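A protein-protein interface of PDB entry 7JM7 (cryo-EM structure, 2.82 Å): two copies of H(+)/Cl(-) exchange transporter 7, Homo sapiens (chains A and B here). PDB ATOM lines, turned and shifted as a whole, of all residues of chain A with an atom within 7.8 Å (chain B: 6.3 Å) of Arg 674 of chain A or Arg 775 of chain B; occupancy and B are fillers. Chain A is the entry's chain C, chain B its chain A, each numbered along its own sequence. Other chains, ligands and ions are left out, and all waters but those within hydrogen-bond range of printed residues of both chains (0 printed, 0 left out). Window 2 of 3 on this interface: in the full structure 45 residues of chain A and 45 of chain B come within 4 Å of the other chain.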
ATOM      1  N   LEU A 638     -26.456  18.551 -14.748  1.00  0.00           N
ATOM      2  CA  LEU A 638     -25.241  17.865 -14.332  1.00  0.00           C
ATOM      3  C   LEU A 638     -24.385  17.635 -15.568  1.00  0.00           C
ATOM      4  O   LEU A 638     -24.859  17.061 -16.552  1.00  0.00           O
ATOM      5  CB  LEU A 638     -25.566  16.526 -13.672  1.00  0.00           C
ATOM      6  CG  LEU A 638     -26.340  16.489 -12.356  1.00  0.00           C
ATOM      7  CD1 LEU A 638     -26.640  15.043 -12.033  1.00  0.00           C
ATOM      8  CD2 LEU A 638     -25.590  17.138 -11.214  1.00  0.00           C
ATOM      9  N   ARG A 640     -21.838  15.818 -17.975  1.00  0.00           N
ATOM     10  CA  ARG A 640     -21.430  14.437 -18.196  1.00  0.00           C
ATOM     11  C   ARG A 640     -20.133  14.116 -17.472  1.00  0.00           C
ATOM     12  O   ARG A 640     -19.828  12.939 -17.248  1.00  0.00           O
ATOM     13  CB  ARG A 640     -21.273  14.183 -19.697  1.00  0.00           C
ATOM     14  CG  ARG A 640     -20.933  12.752 -20.068  1.00  0.00           C
ATOM     15  CD  ARG A 640     -21.013  12.548 -21.572  1.00  0.00           C
ATOM     16  NE  ARG A 640     -21.063  11.134 -21.942  1.00  0.00           N
ATOM     17  CZ  ARG A 640     -22.025  10.561 -22.661  1.00  0.00           C
ATOM     18  NH1 ARG A 640     -23.056  11.262 -23.117  1.00  0.00           N
ATOM     19  NH2 ARG A 640     -21.953   9.266 -22.931  1.00  0.00           N
ATOM     20  N   PRO A 662     -31.202  16.751 -15.859  1.00  0.00           N
ATOM     21  CA  PRO A 662     -30.743  16.437 -17.213  1.00  0.00           C
ATOM     22  C   PRO A 662     -29.247  16.653 -17.355  1.00  0.00           C
ATOM     23  O   PRO A 662     -28.679  17.611 -16.825  1.00  0.00           O
ATOM     24  CB  PRO A 662     -31.535  17.413 -18.089  1.00  0.00           C
ATOM     25  CG  PRO A 662     -31.821  18.560 -17.207  1.00  0.00           C
ATOM     26  CD  PRO A 662     -31.914  18.040 -15.807  1.00  0.00           C
ATOM     27  N   VAL A 663     -28.613  15.751 -18.077  1.00  0.00           N
ATOM     28  CA  VAL A 663     -27.171  15.787 -18.280  1.00  0.00           C
ATOM     29  C   VAL A 663     -26.852  16.700 -19.454  1.00  0.00           C
ATOM     30  O   VAL A 663     -27.665  16.895 -20.363  1.00  0.00           O
ATOM     31  CB  VAL A 663     -26.615  14.367 -18.496  1.00  0.00           C
ATOM     32  CG1 VAL A 663     -25.112  14.407 -18.661  1.00  0.00           C
ATOM     33  CG2 VAL A 663     -27.004  13.483 -17.332  1.00  0.00           C
ATOM     34  N   VAL A 664     -25.647  17.266 -19.431  1.00  0.00           N
ATOM     35  CA  VAL A 664     -25.220  18.245 -20.421  1.00  0.00           C
ATOM     36  C   VAL A 664     -23.735  18.054 -20.692  1.00  0.00           C
ATOM     37  O   VAL A 664     -22.975  17.619 -19.822  1.00  0.00           O
ATOM     38  CB  VAL A 664     -25.518  19.684 -19.950  1.00  0.00           C
ATOM     39  CG1 VAL A 664     -24.784  20.697 -20.806  1.00  0.00           C
ATOM     40  CG2 VAL A 664     -27.015  19.943 -19.978  1.00  0.00           C
ATOM     41  N   GLU A 665     -23.325  18.379 -21.914  1.00  0.00           N
ATOM     42  CA  GLU A 665     -21.930  18.259 -22.315  1.00  0.00           C
ATOM     43  C   GLU A 665     -21.179  19.554 -22.019  1.00  0.00           C
ATOM     44  O   GLU A 665     -19.955  19.559 -21.894  1.00  0.00           O
ATOM     45  CB  GLU A 665     -21.829  17.914 -23.801  1.00  0.00           C
ATOM     46  CG  GLU A 665     -20.407  17.734 -24.312  1.00  0.00           C
ATOM     47  CD  GLU A 665     -19.714  16.539 -23.690  1.00  0.00           C
ATOM     48  OE1 GLU A 665     -20.416  15.606 -23.248  1.00  0.00           O
ATOM     49  OE2 GLU A 665     -18.465  16.532 -23.643  1.00  0.00           O
ATOM     50  N   ALA A 673     -23.595  23.291 -24.472  1.00  0.00           N
ATOM     51  CA  ALA A 673     -24.493  22.698 -23.489  1.00  0.00           C
ATOM     52  C   ALA A 673     -25.536  21.824 -24.174  1.00  0.00           C
ATOM     53  O   ALA A 673     -26.678  22.244 -24.368  1.00  0.00           O
ATOM     54  CB  ALA A 673     -25.167  23.781 -22.667  1.00  0.00           C
ATOM     55  N   ARG A 674     -25.143  20.605 -24.527  1.00  0.00           N
ATOM     56  CA  ARG A 674     -25.975  19.700 -25.306  1.00  0.00           C
ATOM     57  C   ARG A 674     -26.502  18.580 -24.421  1.00  0.00           C
ATOM     58  O   ARG A 674     -25.733  17.942 -23.695  1.00  0.00           O
ATOM     59  CB  ARG A 674     -25.188  19.115 -26.478  1.00  0.00           C
ATOM     60  CG  ARG A 674     -24.990  20.087 -27.621  1.00  0.00           C
ATOM     61  CD  ARG A 674     -24.252  19.439 -28.769  1.00  0.00           C
ATOM     62  NE  ARG A 674     -23.264  20.336 -29.362  1.00  0.00           N
ATOM     63  CZ  ARG A 674     -23.567  21.432 -30.051  1.00  0.00           C
ATOM     64  NH1 ARG A 674     -24.834  21.775 -30.242  1.00  0.00           N
ATOM     65  NH2 ARG A 674     -22.601  22.188 -30.553  1.00  0.00           N
ATOM     66  N   LEU A 675     -27.809  18.341 -24.495  1.00  0.00           N
ATOM     67  CA  LEU A 675     -28.425  17.285 -23.708  1.00  0.00           C
ATOM     68  C   LEU A 675     -27.861  15.927 -24.100  1.00  0.00           C
ATOM     69  O   LEU A 675     -27.704  15.616 -25.284  1.00  0.00           O
ATOM     70  CB  LEU A 675     -29.939  17.301 -23.907  1.00  0.00           C
ATOM     71  CG  LEU A 675     -30.772  16.406 -22.990  1.00  0.00           C
ATOM     72  CD1 LEU A 675     -30.896  17.008 -21.606  1.00  0.00           C
ATOM     73  CD2 LEU A 675     -32.141  16.183 -23.594  1.00  0.00           C
ATOM     74  N   GLN A 676     -27.555  15.113 -23.090  1.00  0.00           N
ATOM     75  CA  GLN A 676     -27.077  13.756 -23.299  1.00  0.00           C
ATOM     76  C   GLN A 676     -27.887  12.709 -22.555  1.00  0.00           C
ATOM     77  O   GLN A 676     -27.751  11.520 -22.866  1.00  0.00           O
ATOM     78  CB  GLN A 676     -25.605  13.627 -22.873  1.00  0.00           C
ATOM     79  CG  GLN A 676     -24.709  14.768 -23.328  1.00  0.00           C
ATOM     80  CD  GLN A 676     -24.408  14.722 -24.809  1.00  0.00           C
ATOM     81  OE1 GLN A 676     -23.940  13.710 -25.329  1.00  0.00           O
ATOM     82  NE2 GLN A 676     -24.675  15.825 -25.499  1.00  0.00           N
ATOM     83  N   GLY A 677     -28.716  13.099 -21.592  1.00  0.00           N
ATOM     84  CA  GLY A 677     -29.501  12.131 -20.853  1.00  0.00           C
ATOM     85  C   GLY A 677     -30.141  12.770 -19.638  1.00  0.00           C
ATOM     86  O   GLY A 677     -30.237  13.993 -19.537  1.00  0.00           O
ATOM     87  N   VAL A 772     -36.174  21.532 -24.975  1.00  0.00           N
ATOM     88  CA  VAL A 772     -34.874  21.707 -25.600  1.00  0.00           C
ATOM     89  C   VAL A 772     -34.989  22.746 -26.709  1.00  0.00           C
ATOM     90  O   VAL A 772     -36.069  23.006 -27.244  1.00  0.00           O
ATOM     91  CB  VAL A 772     -34.338  20.369 -26.151  1.00  0.00           C
ATOM     92  CG1 VAL A 772     -35.069  19.984 -27.414  1.00  0.00           C
ATOM     93  CG2 VAL A 772     -32.856  20.432 -26.394  1.00  0.00           C
ATOM     94  N   ASP A 773     -33.851  23.344 -27.048  1.00  0.00           N
ATOM     95  CA  ASP A 773     -33.783  24.343 -28.103  1.00  0.00           C
ATOM     96  C   ASP A 773     -33.491  23.659 -29.439  1.00  0.00           C
ATOM     97  O   ASP A 773     -33.531  22.433 -29.558  1.00  0.00           O
ATOM     98  CB  ASP A 773     -32.731  25.399 -27.767  1.00  0.00           C
ATOM     99  CG  ASP A 773     -33.089  26.776 -28.299  1.00  0.00           C
ATOM    100  OD1 ASP A 773     -32.241  27.688 -28.202  1.00  0.00           O
ATOM    101  OD2 ASP A 773     -34.208  26.947 -28.824  1.00  0.00           O
ATOM    102  N   ASN A 774     -33.189  24.458 -30.463  1.00  0.00           N
ATOM    103  CA  ASN A 774     -32.977  23.932 -31.804  1.00  0.00           C
ATOM    104  C   ASN A 774     -31.605  23.305 -31.997  1.00  0.00           C
ATOM    105  O   ASN A 774     -31.369  22.694 -33.044  1.00  0.00           O
ATOM    106  CB  ASN A 774     -33.170  25.040 -32.840  1.00  0.00           C
ATOM    107  CG  ASN A 774     -34.582  25.587 -32.853  1.00  0.00           C
ATOM    108  OD1 ASN A 774     -35.476  25.045 -32.204  1.00  0.00           O
ATOM    109  ND2 ASN A 774     -34.791  26.665 -33.601  1.00  0.00           N
ATOM    110  N   ARG A 775     -30.697  23.436 -31.034  1.00  0.00           N
ATOM    111  CA  ARG A 775     -29.362  22.860 -31.129  1.00  0.00           C
ATOM    112  C   ARG A 775     -29.155  21.831 -30.022  1.00  0.00           C
ATOM    113  O   ARG A 775     -28.054  21.659 -29.496  1.00  0.00           O
ATOM    114  CB  ARG A 775     -28.299  23.954 -31.085  1.00  0.00           C
ATOM    115  CG  ARG A 775     -28.505  24.987 -32.183  1.00  0.00           C
ATOM    116  CD  ARG A 775     -27.402  26.027 -32.303  1.00  0.00           C
ATOM    117  NE  ARG A 775     -27.475  27.070 -31.289  1.00  0.00           N
ATOM    118  CZ  ARG A 775     -26.638  28.104 -31.229  1.00  0.00           C
ATOM    119  NH1 ARG A 775     -25.693  28.253 -32.149  1.00  0.00           N
ATOM    120  NH2 ARG A 775     -26.767  29.008 -30.268  1.00  0.00           N
ATOM    121  N   ASN A 776     -30.234  21.130 -29.671  1.00  0.00           N
ATOM    122  CA  ASN A 776     -30.237  20.167 -28.572  1.00  0.00           C
ATOM    123  C   ASN A 776     -29.757  20.840 -27.287  1.00  0.00           C
ATOM    124  O   ASN A 776     -28.977  20.284 -26.512  1.00  0.00           O
ATOM    125  CB  ASN A 776     -29.401  18.933 -28.917  1.00  0.00           C
ATOM    126  CG  ASN A 776     -29.587  17.809 -27.922  1.00  0.00           C
ATOM    127  OD1 ASN A 776     -30.329  17.949 -26.953  1.00  0.00           O
ATOM    128  ND2 ASN A 776     -28.930  16.683 -28.163  1.00  0.00           N
ATOM    129  N   GLN A 777     -30.243  22.060 -27.071  1.00  0.00           N
ATOM    130  CA  GLN A 777     -29.911  22.889 -25.920  1.00  0.00           C
ATOM    131  C   GLN A 777     -30.966  22.726 -24.835  1.00  0.00           C
ATOM    132  O   GLN A 777     -32.159  22.923 -25.090  1.00  0.00           O
ATOM    133  CB  GLN A 777     -29.840  24.364 -26.324  1.00  0.00           C
ATOM    134  CG  GLN A 777     -28.549  25.091 -26.013  1.00  0.00           C
ATOM    135  CD  GLN A 777     -28.608  26.552 -26.422  1.00  0.00           C
ATOM    136  OE1 GLN A 777     -29.611  26.999 -26.979  1.00  0.00           O
ATOM    137  NE2 GLN A 777     -27.563  27.316 -26.111  1.00  0.00           N
ATOM    138  N   VAL A 778     -30.529  22.399 -23.621  1.00  0.00           N
ATOM    139  CA  VAL A 778     -31.464  22.308 -22.503  1.00  0.00           C
ATOM    140  C   VAL A 778     -31.902  23.713 -22.121  1.00  0.00           C
ATOM    141  O   VAL A 778     -31.079  24.549 -21.729  1.00  0.00           O
ATOM    142  CB  VAL A 778     -30.838  21.581 -21.307  1.00  0.00           C
ATOM    143  CG1 VAL A 778     -31.899  21.303 -20.255  1.00  0.00           C
ATOM    144  CG2 VAL A 778     -30.179  20.300 -21.754  1.00  0.00           C
ATOM    145  N   ALA B 673     -27.271  21.897 -40.720  1.00  0.00           N
ATOM    146  CA  ALA B 673     -28.439  21.126 -41.127  1.00  0.00           C
ATOM    147  C   ALA B 673     -29.285  20.755 -39.915  1.00  0.00           C
ATOM    148  O   ALA B 673     -29.215  19.631 -39.420  1.00  0.00           O
ATOM    149  CB  ALA B 673     -28.014  19.877 -41.876  1.00  0.00           C
ATOM    150  N   ARG B 674     -30.092  21.703 -39.449  1.00  0.00           N
ATOM    151  CA  ARG B 674     -30.862  21.554 -38.224  1.00  0.00           C
ATOM    152  C   ARG B 674     -32.334  21.354 -38.552  1.00  0.00           C
ATOM    153  O   ARG B 674     -32.910  22.117 -39.335  1.00  0.00           O
ATOM    154  CB  ARG B 674     -30.687  22.775 -37.323  1.00  0.00           C
ATOM    155  CG  ARG B 674     -29.356  22.813 -36.606  1.00  0.00           C
ATOM    156  CD  ARG B 674     -29.261  24.013 -35.692  1.00  0.00           C
ATOM    157  NE  ARG B 674     -27.942  24.637 -35.742  1.00  0.00           N
ATOM    158  CZ  ARG B 674     -26.830  24.076 -35.276  1.00  0.00           C
ATOM    159  NH1 ARG B 674     -26.869  22.873 -34.720  1.00  0.00           N
ATOM    160  NH2 ARG B 674     -25.675  24.719 -35.366  1.00  0.00           N
ATOM    161  N   LEU B 675     -32.937  20.335 -37.945  1.00  0.00           N
ATOM    162  CA  LEU B 675     -34.347  20.054 -38.167  1.00  0.00           C
ATOM    163  C   LEU B 675     -35.205  21.220 -37.696  1.00  0.00           C
ATOM    164  O   LEU B 675     -34.990  21.778 -36.617  1.00  0.00           O
ATOM    165  CB  LEU B 675     -34.747  18.776 -37.433  1.00  0.00           C
ATOM    166  CG  LEU B 675     -36.133  18.207 -37.731  1.00  0.00           C
ATOM    167  CD1 LEU B 675     -36.159  17.505 -39.072  1.00  0.00           C
ATOM    168  CD2 LEU B 675     -36.548  17.257 -36.630  1.00  0.00           C
ATOM    169  N   VAL B 772     -32.673  11.806 -35.192  1.00  0.00           N
ATOM    170  CA  VAL B 772     -31.871  13.018 -35.155  1.00  0.00           C
ATOM    171  C   VAL B 772     -30.595  12.746 -34.368  1.00  0.00           C
ATOM    172  O   VAL B 772     -30.520  11.826 -33.552  1.00  0.00           O
ATOM    173  CB  VAL B 772     -32.663  14.188 -34.535  1.00  0.00           C
ATOM    174  CG1 VAL B 772     -32.770  14.023 -33.038  1.00  0.00           C
ATOM    175  CG2 VAL B 772     -32.041  15.514 -34.880  1.00  0.00           C
ATOM    176  N   ASP B 773     -29.581  13.567 -34.630  1.00  0.00           N
ATOM    177  CA  ASP B 773     -28.299  13.459 -33.950  1.00  0.00           C
ATOM    178  C   ASP B 773     -28.310  14.331 -32.695  1.00  0.00           C
ATOM    179  O   ASP B 773     -29.349  14.847 -32.276  1.00  0.00           O
ATOM    180  CB  ASP B 773     -27.163  13.845 -34.896  1.00  0.00           C
ATOM    181  CG  ASP B 773     -25.881  13.079 -34.619  1.00  0.00           C
ATOM    182  OD1 ASP B 773     -24.849  13.405 -35.240  1.00  0.00           O
ATOM    183  OD2 ASP B 773     -25.900  12.157 -33.776  1.00  0.00           O
ATOM    184  N   ASN B 774     -27.140  14.506 -32.081  1.00  0.00           N
ATOM    185  CA  ASN B 774     -27.037  15.242 -30.828  1.00  0.00           C
ATOM    186  C   ASN B 774     -27.071  16.752 -31.012  1.00  0.00           C
ATOM    187  O   ASN B 774     -27.141  17.473 -30.011  1.00  0.00           O
ATOM    188  CB  ASN B 774     -25.751  14.856 -30.096  1.00  0.00           C
ATOM    189  CG  ASN B 774     -25.725  13.396 -29.694  1.00  0.00           C
ATOM    190  OD1 ASN B 774     -26.724  12.689 -29.814  1.00  0.00           O
ATOM    191  ND2 ASN B 774     -24.577  12.939 -29.207  1.00  0.00           N
ATOM    192  N   ARG B 775     -27.017  17.251 -32.243  1.00  0.00           N
ATOM    193  CA  ARG B 775     -27.056  18.683 -32.511  1.00  0.00           C
ATOM    194  C   ARG B 775     -28.292  19.030 -33.333  1.00  0.00           C
ATOM    195  O   ARG B 775     -28.281  19.934 -34.170  1.00  0.00           O
ATOM    196  CB  ARG B 775     -25.774  19.134 -33.209  1.00  0.00           C
ATOM    197  CG  ARG B 775     -24.536  18.784 -32.397  1.00  0.00           C
ATOM    198  CD  ARG B 775     -23.229  19.332 -32.950  1.00  0.00           C
ATOM    199  NE  ARG B 775     -22.715  18.577 -34.083  1.00  0.00           N
ATOM    200  CZ  ARG B 775     -21.566  18.852 -34.697  1.00  0.00           C
ATOM    201  NH1 ARG B 775     -20.793  19.837 -34.258  1.00  0.00           N
ATOM    202  NH2 ARG B 775     -21.173  18.120 -35.731  1.00  0.00           N
ATOM    203  N   ASN B 776     -29.381  18.302 -33.079  1.00  0.00           N
ATOM    204  CA  ASN B 776     -30.627  18.440 -33.831  1.00  0.00           C
ATOM    205  C   ASN B 776     -30.358  18.258 -35.323  1.00  0.00           C
ATOM    206  O   ASN B 776     -30.877  18.983 -36.172  1.00  0.00           O
ATOM    207  CB  ASN B 776     -31.307  19.778 -33.532  1.00  0.00           C
ATOM    208  CG  ASN B 776     -32.713  19.850 -34.085  1.00  0.00           C
ATOM    209  OD1 ASN B 776     -33.187  18.907 -34.713  1.00  0.00           O
ATOM    210  ND2 ASN B 776     -33.395  20.960 -33.838  1.00  0.00           N
ATOM    211  N   GLN B 777     -29.531  17.262 -35.633  1.00  0.00           N
ATOM    212  CA  GLN B 777     -29.123  16.918 -36.989  1.00  0.00           C
ATOM    213  C   GLN B 777     -30.005  15.802 -37.533  1.00  0.00           C
ATOM    214  O   GLN B 777     -30.125  14.742 -36.910  1.00  0.00           O
ATOM    215  CB  GLN B 777     -27.665  16.451 -37.010  1.00  0.00           C
ATOM    216  CG  GLN B 777     -26.729  17.192 -37.942  1.00  0.00           C
ATOM    217  CD  GLN B 777     -25.324  16.619 -37.905  1.00  0.00           C
ATOM    218  OE1 GLN B 777     -25.053  15.691 -37.144  1.00  0.00           O
ATOM    219  NE2 GLN B 777     -24.436  17.128 -38.756  1.00  0.00           N
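Among the printed residues, no Asp or Glu carboxylate lies within 4 Å of a Lys or Arg side-chain nitrogen of the other chain.
Arg 674 of chain A touches Asn 774 of chain B, and with the chains exchanged Asn 774 of chain A touches Arg 674 of chain B.
Arg 674 of chain A touches Arg 775 of chain B, and with the chains exchanged Arg 775 of chain A touches Arg 674 of chain B.
Asn 774 of chain A touches Asn 776 of chain B, and with the chains exchanged Asn 776 of chain A touches Asn 774 of chain B.
Positions printed for both chains: 673, 674, 675, 772, 773, 774, 775, 776 and 777.
Of the 6 pairs that touch across the chains among the printed residues, 6 have their exchanged pair printed and touching as well.
The side-chain amide nitrogen (ND2) of Asn 776 of chain A is in hydrogen-bond range of the backbone carbonyl oxygen (O) of Asn 774 of chain B (2.7 Å).
The backbone carbonyl oxygen of Asn 774 of chain A lies within hydrogen-bond range of the side-chain amide nitrogen of Asn 776 of chain B (2.8 Å).
Of chain B, only Asn 774 and Arg 775 come within 4 Å of Arg 674 of chain A.
Arg 775 of chain B touches just one residue of chain A: Arg 674.
Printed residues of chain B within 4 Å of Asn 776 of chain A: Asn 774 (2.7 Å).
Printed residues of chain B within 4 Å of Arg 775 of chain A: Arg 674 (3.6 Å).
Arg 674 of chain A touches Asn 774 of chain B (CD to O, 3.7 Å).
Arg 674 of chain A touches Arg 775 of chain B.
Asn 774 of chain A touches Arg 674 of chain B (O to CD, 3.6 Å).
Arg 775 of chain A touches Arg 674 of chain B.
N of Glu 665 of chain A is in hydrogen-bond range of O of Arg 674 of chain A.
O of Arg 775 of chain B is in hydrogen-bond range of NH1 of Arg 674 of chain B (3.3 Å).
The side-chain amide nitrogen (NE2) of Gln 676 of chain A is in hydrogen-bond range of the backbone carbonyl oxygen (O) of Arg 674 of chain A (3.0 Å).
O of Arg 775 of chain A is in hydrogen-bond range of NH1 of Arg 674 of chain A, 3.3 Å away.
N of Leu 675 of chain A lies within hydrogen-bond range of O of Asn 776 of chain A, at 3.0 Å.
The backbone NH (N) of Leu 675 of chain B lies within hydrogen-bond range of the backbone carbonyl oxygen (O) of Asn 776 of chain B (3.0 Å).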
